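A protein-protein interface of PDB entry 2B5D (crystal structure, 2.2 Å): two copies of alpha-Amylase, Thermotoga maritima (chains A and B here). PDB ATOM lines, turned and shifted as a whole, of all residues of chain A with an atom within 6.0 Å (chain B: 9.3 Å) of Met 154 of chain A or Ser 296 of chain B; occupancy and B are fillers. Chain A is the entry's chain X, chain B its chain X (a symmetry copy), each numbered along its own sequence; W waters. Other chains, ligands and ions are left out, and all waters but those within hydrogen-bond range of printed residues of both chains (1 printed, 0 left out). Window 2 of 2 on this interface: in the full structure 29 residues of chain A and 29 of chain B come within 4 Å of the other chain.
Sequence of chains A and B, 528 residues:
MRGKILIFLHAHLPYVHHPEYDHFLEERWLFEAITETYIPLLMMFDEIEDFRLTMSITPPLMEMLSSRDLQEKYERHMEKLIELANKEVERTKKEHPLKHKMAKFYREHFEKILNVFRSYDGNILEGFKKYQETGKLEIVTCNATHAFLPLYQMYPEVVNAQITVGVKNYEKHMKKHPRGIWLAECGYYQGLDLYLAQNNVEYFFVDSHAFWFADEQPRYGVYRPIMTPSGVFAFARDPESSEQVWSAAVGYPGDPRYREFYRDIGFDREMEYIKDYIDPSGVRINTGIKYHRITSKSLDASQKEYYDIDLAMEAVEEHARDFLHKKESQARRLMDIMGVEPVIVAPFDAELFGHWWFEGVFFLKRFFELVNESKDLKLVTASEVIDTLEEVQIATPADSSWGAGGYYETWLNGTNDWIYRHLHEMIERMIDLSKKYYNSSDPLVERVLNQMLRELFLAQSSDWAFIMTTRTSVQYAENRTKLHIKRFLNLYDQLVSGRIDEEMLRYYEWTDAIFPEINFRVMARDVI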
ATOM      1  N   PRO A 150      21.021  25.840  -3.613  1.00  0.00           N
ATOM      2  CA  PRO A 150      20.785  25.249  -2.283  1.00  0.00           C
ATOM      3  C   PRO A 150      20.049  26.154  -1.296  1.00  0.00           C
ATOM      4  O   PRO A 150      19.474  25.669  -0.301  1.00  0.00           O
ATOM      5  CB  PRO A 150      22.216  24.947  -1.755  1.00  0.00           C
ATOM      6  CG  PRO A 150      23.056  24.935  -2.926  1.00  0.00           C
ATOM      7  CD  PRO A 150      22.461  25.879  -3.938  1.00  0.00           C
ATOM      8  N   LEU A 151      20.094  27.460  -1.509  1.00  0.00           N
ATOM      9  CA  LEU A 151      19.283  28.311  -0.673  1.00  0.00           C
ATOM     10  C   LEU A 151      17.769  28.074  -0.900  1.00  0.00           C
ATOM     11  O   LEU A 151      16.979  28.177   0.025  1.00  0.00           O
ATOM     12  CB  LEU A 151      19.650  29.786  -0.907  1.00  0.00           C
ATOM     13  CG  LEU A 151      18.985  30.788   0.056  1.00  0.00           C
ATOM     14  CD1 LEU A 151      19.275  30.473   1.554  1.00  0.00           C
ATOM     15  CD2 LEU A 151      19.366  32.234  -0.355  1.00  0.00           C
ATOM     16  N   TYR A 152      17.398  27.727  -2.123  1.00  0.00           N
ATOM     17  CA  TYR A 152      16.004  27.534  -2.545  1.00  0.00           C
ATOM     18  C   TYR A 152      15.508  26.069  -2.663  1.00  0.00           C
ATOM     19  O   TYR A 152      14.473  25.806  -3.298  1.00  0.00           O
ATOM     20  CB  TYR A 152      15.830  28.213  -3.893  1.00  0.00           C
ATOM     21  CG  TYR A 152      16.150  29.674  -3.747  1.00  0.00           C
ATOM     22  CD1 TYR A 152      15.267  30.519  -3.040  1.00  0.00           C
ATOM     23  CD2 TYR A 152      17.361  30.219  -4.261  1.00  0.00           C
ATOM     24  CE1 TYR A 152      15.545  31.838  -2.860  1.00  0.00           C
ATOM     25  CE2 TYR A 152      17.656  31.590  -4.075  1.00  0.00           C
ATOM     26  CZ  TYR A 152      16.738  32.381  -3.374  1.00  0.00           C
ATOM     27  OH  TYR A 152      16.957  33.729  -3.183  1.00  0.00           O
ATOM     28  N   GLN A 153      16.226  25.132  -2.047  1.00  0.00           N
ATOM     29  CA  GLN A 153      15.941  23.709  -2.278  1.00  0.00           C
ATOM     30  C   GLN A 153      14.533  23.277  -1.802  1.00  0.00           C
ATOM     31  O   GLN A 153      14.010  22.250  -2.239  1.00  0.00           O
ATOM     32  CB  GLN A 153      16.997  22.818  -1.662  1.00  0.00           C
ATOM     33  CG  GLN A 153      17.105  22.858  -0.183  1.00  0.00           C
ATOM     34  CD  GLN A 153      18.359  22.130   0.284  1.00  0.00           C
ATOM     35  OE1 GLN A 153      18.297  20.985   0.720  1.00  0.00           O
ATOM     36  NE2 GLN A 153      19.505  22.778   0.147  1.00  0.00           N
ATOM     37  N   MET A 154      13.958  24.073  -0.906  1.00  0.00           N
ATOM     38  CA  MET A 154      12.630  23.802  -0.433  1.00  0.00           C
ATOM     39  C   MET A 154      11.541  24.323  -1.372  1.00  0.00           C
ATOM     40  O   MET A 154      10.383  24.143  -1.102  1.00  0.00           O
ATOM     41  CB  MET A 154      12.439  24.313   0.993  1.00  0.00           C
ATOM     42  CG  MET A 154      11.182  23.753   1.583  1.00  0.00           C
ATOM     43  SD  MET A 154      11.276  23.782   3.354  1.00  0.00           S
ATOM     44  CE  MET A 154       9.635  23.118   3.728  1.00  0.00           C
ATOM     45  N   TYR A 155      11.939  24.903  -2.499  1.00  0.00           N
ATOM     46  CA  TYR A 155      11.066  25.515  -3.467  1.00  0.00           C
ATOM     47  C   TYR A 155      11.498  24.973  -4.803  1.00  0.00           C
ATOM     48  O   TYR A 155      12.028  25.715  -5.625  1.00  0.00           O
ATOM     49  CB  TYR A 155      11.192  27.068  -3.402  1.00  0.00           C
ATOM     50  CG  TYR A 155      11.018  27.611  -1.980  1.00  0.00           C
ATOM     51  CD1 TYR A 155       9.750  27.904  -1.473  1.00  0.00           C
ATOM     52  CD2 TYR A 155      12.131  27.817  -1.139  1.00  0.00           C
ATOM     53  CE1 TYR A 155       9.572  28.390  -0.150  1.00  0.00           C
ATOM     54  CE2 TYR A 155      11.977  28.286   0.188  1.00  0.00           C
ATOM     55  CZ  TYR A 155      10.701  28.599   0.676  1.00  0.00           C
ATOM     56  OH  TYR A 155      10.545  29.065   1.990  1.00  0.00           O
ATOM     57  N   PRO A 156      11.303  23.644  -5.020  1.00  0.00           N
ATOM     58  CA  PRO A 156      11.711  22.945  -6.237  1.00  0.00           C
ATOM     59  C   PRO A 156      11.203  23.612  -7.497  1.00  0.00           C
ATOM     60  O   PRO A 156      11.903  23.572  -8.508  1.00  0.00           O
ATOM     61  CB  PRO A 156      11.070  21.570  -6.115  1.00  0.00           C
ATOM     62  CG  PRO A 156      10.442  21.443  -4.775  1.00  0.00           C
ATOM     63  CD  PRO A 156      10.729  22.724  -4.007  1.00  0.00           C
ATOM     64  N   GLU A 157      10.015  24.233  -7.454  1.00  0.00           N
ATOM     65  CA  GLU A 157       9.493  24.955  -8.630  1.00  0.00           C
ATOM     66  C   GLU A 157      10.445  26.076  -9.080  1.00  0.00           C
ATOM     67  O   GLU A 157      10.677  26.278 -10.298  1.00  0.00           O
ATOM     68  CB  GLU A 157       8.085  25.558  -8.360  1.00  0.00           C
ATOM     69  CG  GLU A 157       6.959  24.573  -7.902  1.00  0.00           C
ATOM     70  CD  GLU A 157       7.090  24.199  -6.444  1.00  0.00           C
ATOM     71  OE1 GLU A 157       6.150  23.608  -5.913  1.00  0.00           O
ATOM     72  OE2 GLU A 157       8.147  24.470  -5.797  1.00  0.00           O
ATOM     73  N   VAL A 159      13.700  26.460  -8.247  1.00  0.00           N
ATOM     74  CA  VAL A 159      14.931  25.767  -8.651  1.00  0.00           C
ATOM     75  C   VAL A 159      14.919  25.258 -10.091  1.00  0.00           C
ATOM     76  O   VAL A 159      15.832  25.563 -10.878  1.00  0.00           O
ATOM     77  CB  VAL A 159      15.275  24.660  -7.676  1.00  0.00           C
ATOM     78  CG1 VAL A 159      16.526  23.859  -8.164  1.00  0.00           C
ATOM     79  CG2 VAL A 159      15.511  25.232  -6.254  1.00  0.00           C
ATOM     80  N   TYR A 189      22.907  20.399  -4.128  1.00  0.00           N
ATOM     81  CA  TYR A 189      22.286  19.644  -3.030  1.00  0.00           C
ATOM     82  C   TYR A 189      21.698  18.341  -3.594  1.00  0.00           C
ATOM     83  O   TYR A 189      21.426  18.215  -4.787  1.00  0.00           O
ATOM     84  CB  TYR A 189      21.196  20.461  -2.299  1.00  0.00           C
ATOM     85  CG  TYR A 189      20.002  20.815  -3.152  1.00  0.00           C
ATOM     86  CD1 TYR A 189      20.023  21.955  -3.973  1.00  0.00           C
ATOM     87  CD2 TYR A 189      18.868  20.004  -3.159  1.00  0.00           C
ATOM     88  CE1 TYR A 189      18.902  22.304  -4.773  1.00  0.00           C
ATOM     89  CE2 TYR A 189      17.761  20.322  -3.929  1.00  0.00           C
ATOM     90  CZ  TYR A 189      17.778  21.474  -4.725  1.00  0.00           C
ATOM     91  OH  TYR A 189      16.693  21.756  -5.488  1.00  0.00           O
ATOM     92  N   ALA B 248      26.308  25.349   7.933  1.00  0.00           N
ATOM     93  CA  ALA B 248      24.867  25.256   8.129  1.00  0.00           C
ATOM     94  C   ALA B 248      24.133  25.001   6.818  1.00  0.00           C
ATOM     95  O   ALA B 248      23.059  24.384   6.796  1.00  0.00           O
ATOM     96  CB  ALA B 248      24.341  26.530   8.762  1.00  0.00           C
ATOM     97  N   GLY B 254      23.615  22.300   9.970  1.00  0.00           N
ATOM     98  CA  GLY B 254      22.356  22.646   9.317  1.00  0.00           C
ATOM     99  C   GLY B 254      21.208  21.659   9.509  1.00  0.00           C
ATOM    100  O   GLY B 254      20.129  21.844   8.944  1.00  0.00           O
ATOM    101  N   ASP B 255      21.417  20.616  10.318  1.00  0.00           N
ATOM    102  CA  ASP B 255      20.371  19.650  10.644  1.00  0.00           C
ATOM    103  C   ASP B 255      19.145  20.305  11.296  1.00  0.00           C
ATOM    104  O   ASP B 255      19.277  21.081  12.256  1.00  0.00           O
ATOM    105  CB  ASP B 255      20.935  18.566  11.562  1.00  0.00           C
ATOM    106  CG  ASP B 255      19.994  17.382  11.735  1.00  0.00           C
ATOM    107  OD1 ASP B 255      19.011  17.526  12.500  1.00  0.00           O
ATOM    108  OD2 ASP B 255      20.252  16.297  11.137  1.00  0.00           O
ATOM    109  N   PRO B 256      17.931  19.973  10.790  1.00  0.00           N
ATOM    110  CA  PRO B 256      16.702  20.557  11.339  1.00  0.00           C
ATOM    111  C   PRO B 256      16.476  20.376  12.843  1.00  0.00           C
ATOM    112  O   PRO B 256      15.701  21.138  13.418  1.00  0.00           O
ATOM    113  CB  PRO B 256      15.577  19.920  10.500  1.00  0.00           C
ATOM    114  CG  PRO B 256      16.187  18.814   9.742  1.00  0.00           C
ATOM    115  CD  PRO B 256      17.669  19.058   9.662  1.00  0.00           C
ATOM    116  N   ARG B 257      17.151  19.429  13.492  1.00  0.00           N
ATOM    117  CA  ARG B 257      16.972  19.183  14.966  1.00  0.00           C
ATOM    118  C   ARG B 257      17.826  20.093  15.829  1.00  0.00           C
ATOM    119  O   ARG B 257      17.757  20.056  17.074  1.00  0.00           O
ATOM    120  CB  ARG B 257      17.333  17.737  15.352  1.00  0.00           C
ATOM    121  CG  ARG B 257      16.412  16.650  14.773  1.00  0.00           C
ATOM    122  CD  ARG B 257      17.056  15.287  14.944  1.00  0.00           C
ATOM    123  NE  ARG B 257      18.054  15.040  13.907  1.00  0.00           N
ATOM    124  CZ  ARG B 257      18.708  13.894  13.731  1.00  0.00           C
ATOM    125  NH1 ARG B 257      19.604  13.796  12.752  1.00  0.00           N
ATOM    126  NH2 ARG B 257      18.481  12.861  14.539  1.00  0.00           N
ATOM    127  N   TYR B 258      18.685  20.869  15.176  1.00  0.00           N
ATOM    128  CA  TYR B 258      19.632  21.695  15.903  1.00  0.00           C
ATOM    129  C   TYR B 258      19.053  23.076  16.206  1.00  0.00           C
ATOM    130  O   TYR B 258      18.193  23.581  15.484  1.00  0.00           O
ATOM    131  CB  TYR B 258      20.965  21.794  15.155  1.00  0.00           C
ATOM    132  CG  TYR B 258      21.873  20.571  15.259  1.00  0.00           C
ATOM    133  CD1 TYR B 258      22.556  20.113  14.151  1.00  0.00           C
ATOM    134  CD2 TYR B 258      22.042  19.890  16.462  1.00  0.00           C
ATOM    135  CE1 TYR B 258      23.382  19.016  14.222  1.00  0.00           C
ATOM    136  CE2 TYR B 258      22.872  18.787  16.558  1.00  0.00           C
ATOM    137  CZ  TYR B 258      23.541  18.354  15.440  1.00  0.00           C
ATOM    138  OH  TYR B 258      24.380  17.256  15.508  1.00  0.00           O
ATOM    139  N   GLU B 260      18.283  26.826  16.433  1.00  0.00           N
ATOM    140  CA  GLU B 260      18.311  27.946  15.496  1.00  0.00           C
ATOM    141  C   GLU B 260      18.981  29.164  16.127  1.00  0.00           C
ATOM    142  O   GLU B 260      18.610  29.588  17.221  1.00  0.00           O
ATOM    143  CB  GLU B 260      16.885  28.278  15.066  1.00  0.00           C
ATOM    144  CG  GLU B 260      16.741  29.543  14.238  1.00  0.00           C
ATOM    145  CD  GLU B 260      17.451  29.449  12.903  1.00  0.00           C
ATOM    146  OE1 GLU B 260      18.390  30.238  12.679  1.00  0.00           O
ATOM    147  OE2 GLU B 260      17.084  28.573  12.086  1.00  0.00           O
ATOM    148  N   HIS B 292      13.980  27.944  19.437  1.00  0.00           N
ATOM    149  CA  HIS B 292      13.628  27.240  18.204  1.00  0.00           C
ATOM    150  C   HIS B 292      14.757  26.374  17.657  1.00  0.00           C
ATOM    151  O   HIS B 292      15.946  26.613  17.943  1.00  0.00           O
ATOM    152  CB  HIS B 292      13.127  28.232  17.164  1.00  0.00           C
ATOM    153  CG  HIS B 292      11.980  29.079  17.654  1.00  0.00           C
ATOM    154  ND1 HIS B 292      12.143  30.102  18.572  1.00  0.00           N
ATOM    155  CD2 HIS B 292      10.656  29.032  17.376  1.00  0.00           C
ATOM    156  CE1 HIS B 292      10.972  30.666  18.808  1.00  0.00           C
ATOM    157  NE2 HIS B 292      10.056  30.039  18.090  1.00  0.00           N
ATOM    158  N   ARG B 293      14.361  25.324  16.940  1.00  0.00           N
ATOM    159  CA  ARG B 293      15.302  24.530  16.185  1.00  0.00           C
ATOM    160  C   ARG B 293      15.261  24.994  14.720  1.00  0.00           C
ATOM    161  O   ARG B 293      14.303  25.644  14.299  1.00  0.00           O
ATOM    162  CB  ARG B 293      14.984  23.034  16.308  1.00  0.00           C
ATOM    163  CG  ARG B 293      13.559  22.645  15.946  1.00  0.00           C
ATOM    164  CD  ARG B 293      13.284  21.184  16.277  1.00  0.00           C
ATOM    165  NE  ARG B 293      12.026  20.751  15.679  1.00  0.00           N
ATOM    166  CZ  ARG B 293      11.896  20.199  14.473  1.00  0.00           C
ATOM    167  NH1 ARG B 293      12.954  19.989  13.697  1.00  0.00           N
ATOM    168  NH2 ARG B 293      10.691  19.874  14.035  1.00  0.00           N
ATOM    169  N   ILE B 294      16.279  24.632  13.946  1.00  0.00           N
ATOM    170  CA  ILE B 294      16.363  25.058  12.547  1.00  0.00           C
ATOM    171  C   ILE B 294      15.111  24.652  11.748  1.00  0.00           C
ATOM    172  O   ILE B 294      14.689  25.402  10.859  1.00  0.00           O
ATOM    173  CB  ILE B 294      17.699  24.583  11.874  1.00  0.00           C
ATOM    174  CG1 ILE B 294      18.908  25.222  12.572  1.00  0.00           C
ATOM    175  CG2 ILE B 294      17.718  24.864  10.345  1.00  0.00           C
ATOM    176  CD1 ILE B 294      20.215  24.531  12.319  1.00  0.00           C
ATOM    177  N   THR B 295      14.571  23.455  12.033  1.00  0.00           N
ATOM    178  CA  THR B 295      13.261  22.972  11.537  1.00  0.00           C
ATOM    179  C   THR B 295      13.230  22.473  10.087  1.00  0.00           C
ATOM    180  O   THR B 295      12.679  21.397   9.800  1.00  0.00           O
ATOM    181  CB  THR B 295      12.161  24.054  11.717  1.00  0.00           C
ATOM    182  OG1 THR B 295      12.099  24.430  13.091  1.00  0.00           O
ATOM    183  CG2 THR B 295      10.794  23.541  11.272  1.00  0.00           C
ATOM    184  N   SER B 296      13.781  23.266   9.157  1.00  0.00           N
ATOM    185  CA  SER B 296      13.668  22.948   7.740  1.00  0.00           C
ATOM    186  C   SER B 296      14.434  23.978   6.944  1.00  0.00           C
ATOM    187  O   SER B 296      14.907  24.949   7.502  1.00  0.00           O
ATOM    188  CB  SER B 296      12.205  22.991   7.306  1.00  0.00           C
ATOM    189  OG  SER B 296      11.844  24.318   6.942  1.00  0.00           O
ATOM    190  N   LYS B 297      14.508  23.780   5.636  1.00  0.00           N
ATOM    191  CA  LYS B 297      15.183  24.700   4.732  1.00  0.00           C
ATOM    192  C   LYS B 297      14.351  25.900   4.346  1.00  0.00           C
ATOM    193  O   LYS B 297      14.683  26.606   3.391  1.00  0.00           O
ATOM    194  CB  LYS B 297      15.605  23.965   3.457  1.00  0.00           C
ATOM    195  CG  LYS B 297      16.674  22.937   3.700  1.00  0.00           C
ATOM    196  CD  LYS B 297      17.973  23.566   4.197  1.00  0.00           C
ATOM    197  CE  LYS B 297      19.111  22.516   4.172  1.00  0.00           C
ATOM    198  NZ  LYS B 297      20.421  23.213   4.391  1.00  0.00           N
ATOM    199  N   SER B 298      13.239  26.117   5.050  1.00  0.00           N
ATOM    200  CA  SER B 298      12.337  27.195   4.673  1.00  0.00           C
ATOM    201  C   SER B 298      12.995  28.554   4.873  1.00  0.00           C
ATOM    202  O   SER B 298      13.752  28.751   5.807  1.00  0.00           O
ATOM    203  CB  SER B 298      11.024  27.123   5.437  1.00  0.00           C
ATOM    204  OG  SER B 298      10.131  28.063   4.914  1.00  0.00           O
ATOM    205  N   LEU B 299      12.693  29.463   3.956  1.00  0.00           N
ATOM    206  CA  LEU B 299      13.033  30.866   4.041  1.00  0.00           C
ATOM    207  C   LEU B 299      12.085  31.608   4.983  1.00  0.00           C
ATOM    208  O   LEU B 299      12.366  32.730   5.374  1.00  0.00           O
ATOM    209  CB  LEU B 299      12.927  31.459   2.643  1.00  0.00           C
ATOM    210  CG  LEU B 299      14.207  31.604   1.840  1.00  0.00           C
ATOM    211  CD1 LEU B 299      15.360  30.733   2.367  1.00  0.00           C
ATOM    212  CD2 LEU B 299      13.963  31.377   0.400  1.00  0.00           C
ATOM    213  N   ASP B 300      10.952  30.983   5.312  1.00  0.00           N
ATOM    214  CA  ASP B 300       9.986  31.529   6.246  1.00  0.00           C
ATOM    215  C   ASP B 300      10.363  31.181   7.683  1.00  0.00           C
ATOM    216  O   ASP B 300       9.955  30.140   8.208  1.00  0.00           O
ATOM    217  CB  ASP B 300       8.579  31.024   5.915  1.00  0.00           C
ATOM    218  CG  ASP B 300       7.492  31.623   6.819  1.00  0.00           C
ATOM    219  OD1 ASP B 300       7.810  32.427   7.717  1.00  0.00           O
ATOM    220  OD2 ASP B 300       6.310  31.250   6.638  1.00  0.00           O
ATOM    221  N   ALA B 301      11.129  32.074   8.314  1.00  0.00           N
ATOM    222  CA  ALA B 301      11.639  31.850   9.670  1.00  0.00           C
ATOM    223  C   ALA B 301      10.545  31.764  10.742  1.00  0.00           C
ATOM    224  O   ALA B 301      10.768  31.205  11.813  1.00  0.00           O
ATOM    225  CB  ALA B 301      12.694  32.896  10.041  1.00  0.00           C
ATOM    226  N   SER B 302       9.361  32.297  10.432  1.00  0.00           N
ATOM    227  CA  SER B 302       8.228  32.244  11.359  1.00  0.00           C
ATOM    228  C   SER B 302       7.657  30.830  11.540  1.00  0.00           C
ATOM    229  O   SER B 302       6.957  30.546  12.516  1.00  0.00           O
ATOM    230  CB  SER B 302       7.134  33.226  10.918  1.00  0.00           C
ATOM    231  OG  SER B 302       6.300  32.649   9.925  1.00  0.00           O
ATOM    232  N   GLN B 303       7.977  29.935  10.613  1.00  0.00           N
ATOM    233  CA  GLN B 303       7.461  28.572  10.672  1.00  0.00           C
ATOM    234  C   GLN B 303       8.319  27.610  11.507  1.00  0.00           C
ATOM    235  O   GLN B 303       8.089  26.397  11.496  1.00  0.00           O
ATOM    236  CB  GLN B 303       7.267  28.035   9.258  1.00  0.00           C
ATOM    237  CG  GLN B 303       6.184  28.779   8.450  1.00  0.00           C
ATOM    238  CD  GLN B 303       5.860  28.058   7.149  1.00  0.00           C
ATOM    239  OE1 GLN B 303       5.761  26.828   7.128  1.00  0.00           O
ATOM    240  NE2 GLN B 303       5.738  28.812   6.051  1.00  0.00           N
ATOM    241  N   LYS B 304       9.278  28.169  12.245  1.00  0.00           N
ATOM    242  CA  LYS B 304      10.226  27.403  13.038  1.00  0.00           C
ATOM    243  C   LYS B 304       9.654  26.797  14.308  1.00  0.00           C
ATOM    244  O   LYS B 304       8.995  27.469  15.098  1.00  0.00           O
ATOM    245  CB  LYS B 304      11.473  28.251  13.365  1.00  0.00           C
ATOM    246  CG  LYS B 304      12.313  28.463  12.121  1.00  0.00           C
ATOM    247  CD  LYS B 304      13.711  28.877  12.420  1.00  0.00           C
ATOM    248  CE  LYS B 304      14.389  29.329  11.143  1.00  0.00           C
ATOM    249  NZ  LYS B 304      15.059  28.223  10.384  1.00  0.00           N
ATOM    250  N   GLU B 305       9.947  25.522  14.509  1.00  0.00           N
ATOM    251  CA  GLU B 305       9.456  24.805  15.658  1.00  0.00           C
ATOM    252  C   GLU B 305      10.358  24.930  16.859  1.00  0.00           C
ATOM    253  O   GLU B 305      11.537  25.251  16.740  1.00  0.00           O
ATOM    254  CB  GLU B 305       9.223  23.343  15.296  1.00  0.00           C
ATOM    255  CG  GLU B 305       7.918  23.204  14.565  1.00  0.00           C
ATOM    256  CD  GLU B 305       7.755  21.878  13.908  1.00  0.00           C
ATOM    257  OE1 GLU B 305       7.468  21.890  12.688  1.00  0.00           O
ATOM    258  OE2 GLU B 305       7.912  20.831  14.608  1.00  0.00           O
HETATM  259  O   HOH W   1      14.996  26.452   0.822  1.00  0.00           O
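Water W1 lies within hydrogen-bond range of the backbone carbonyl oxygen (O) of Lys 297 of chain B (2.6 Å), the backbone carbonyl oxygen (O) of Leu 151 of chain A (2.7 Å), the backbone NH (N) of Met 154 of chain A (3.1 Å) and the backbone NH (N) of Gln 153 of chain A (3.4 Å).
The backbone NH of Asp 300 of chain B sits at hydrogen-bond distance from the side-chain hydroxyl of Ser 298 of chain B, at 3.1 Å.
NE2 of Gln 303 of chain B is in hydrogen-bond range of OD2 of Asp 300 of chain B (2.6 Å).
The side-chain hydroxyl (OG) of Ser 302 of chain B sits at hydrogen-bond distance from the side-chain carboxylate (OD1) of Asp 300 of chain B, at 2.7 Å.
The side-chain hydroxyl (OG) of Ser 296 of chain B sits at hydrogen-bond distance from the backbone NH (N) of Ser 298 of chain B.
NE2 of Gln 153 of chain A lies within hydrogen-bond range of O of Pro 150 of chain A (2.9 Å).
Among the printed residues, merely in contact across the chains: Tyr 152 of chain A with Leu 299 of chain B, Leu 151 of chain A with Leu 299 of chain B, Tyr 155 of chain A with Asp 300 of chain B, Gln 153 of chain A with Lys 297 of chain B and Met 154 of chain A with Lys 297 of chain B.
No position is printed for both chains.
Printed residues of chain B within 4 Å of Leu 151 of chain A: Leu 299.
Of the printed residues of chain B, Gln 153 of chain A touches Lys 297 (3.9 Å).
Printed residues of chain B within 4 Å of Met 154 of chain A: Ser 296, Lys 297 and Ser 298.
Of chain B, only Ser 298, Leu 299 and Asp 300 come within 4 Å of Tyr 155 of chain A.
Tyr 189 of chain A touches none of the printed residues of chain B.
Of chain A, only Met 154 (3.7 Å) comes within 4 Å of Ser 296 of chain B.
Of the printed residues of chain A, Lys 297 of chain B touches Gln 153 (3.9 Å) and Met 154 (3.9 Å).
Ala 301 of chain B touches none of the printed residues of chain A.
The nearest residue of chain B that does not touch Met 154 of chain A is Leu 299 of chain B (5.9 Å).
Of the 10 printed residues of chain A, 5 touch a printed residue of chain B.
Printed residues of chain A that touch a printed residue of chain B: Leu 151, Tyr 152, Gln 153, Met 154 and Tyr 155.
Of the 21 printed residues of chain B, 5 touch a printed residue of chain A.
Among the printed residues, 9 pairs touch across the chains.
Among the printed residues, no Asp or Glu carboxylate lies within 4 Å of a Lys or Arg side-chain nitrogen of the other chain.
The side-chain sulfur of Met 154 of chain A sits at hydrogen-bond distance from the side-chain hydroxyl of Ser 296 of chain B, 3.7 Å away.
The side-chain hydroxyl (OG) of Ser 298 of chain B lies within hydrogen-bond range of the side-chain hydroxyl (OH) of Tyr 155 of chain A, at 3.1 Å.
The backbone NH of Ser 298 of chain B is in hydrogen-bond range of the side-chain sulfur of Met 154 of chain A.
The side-chain hydroxyl of Tyr 155 of chain A is in hydrogen-bond range of the backbone NH of Leu 299 of chain B, at 2.9 Å.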
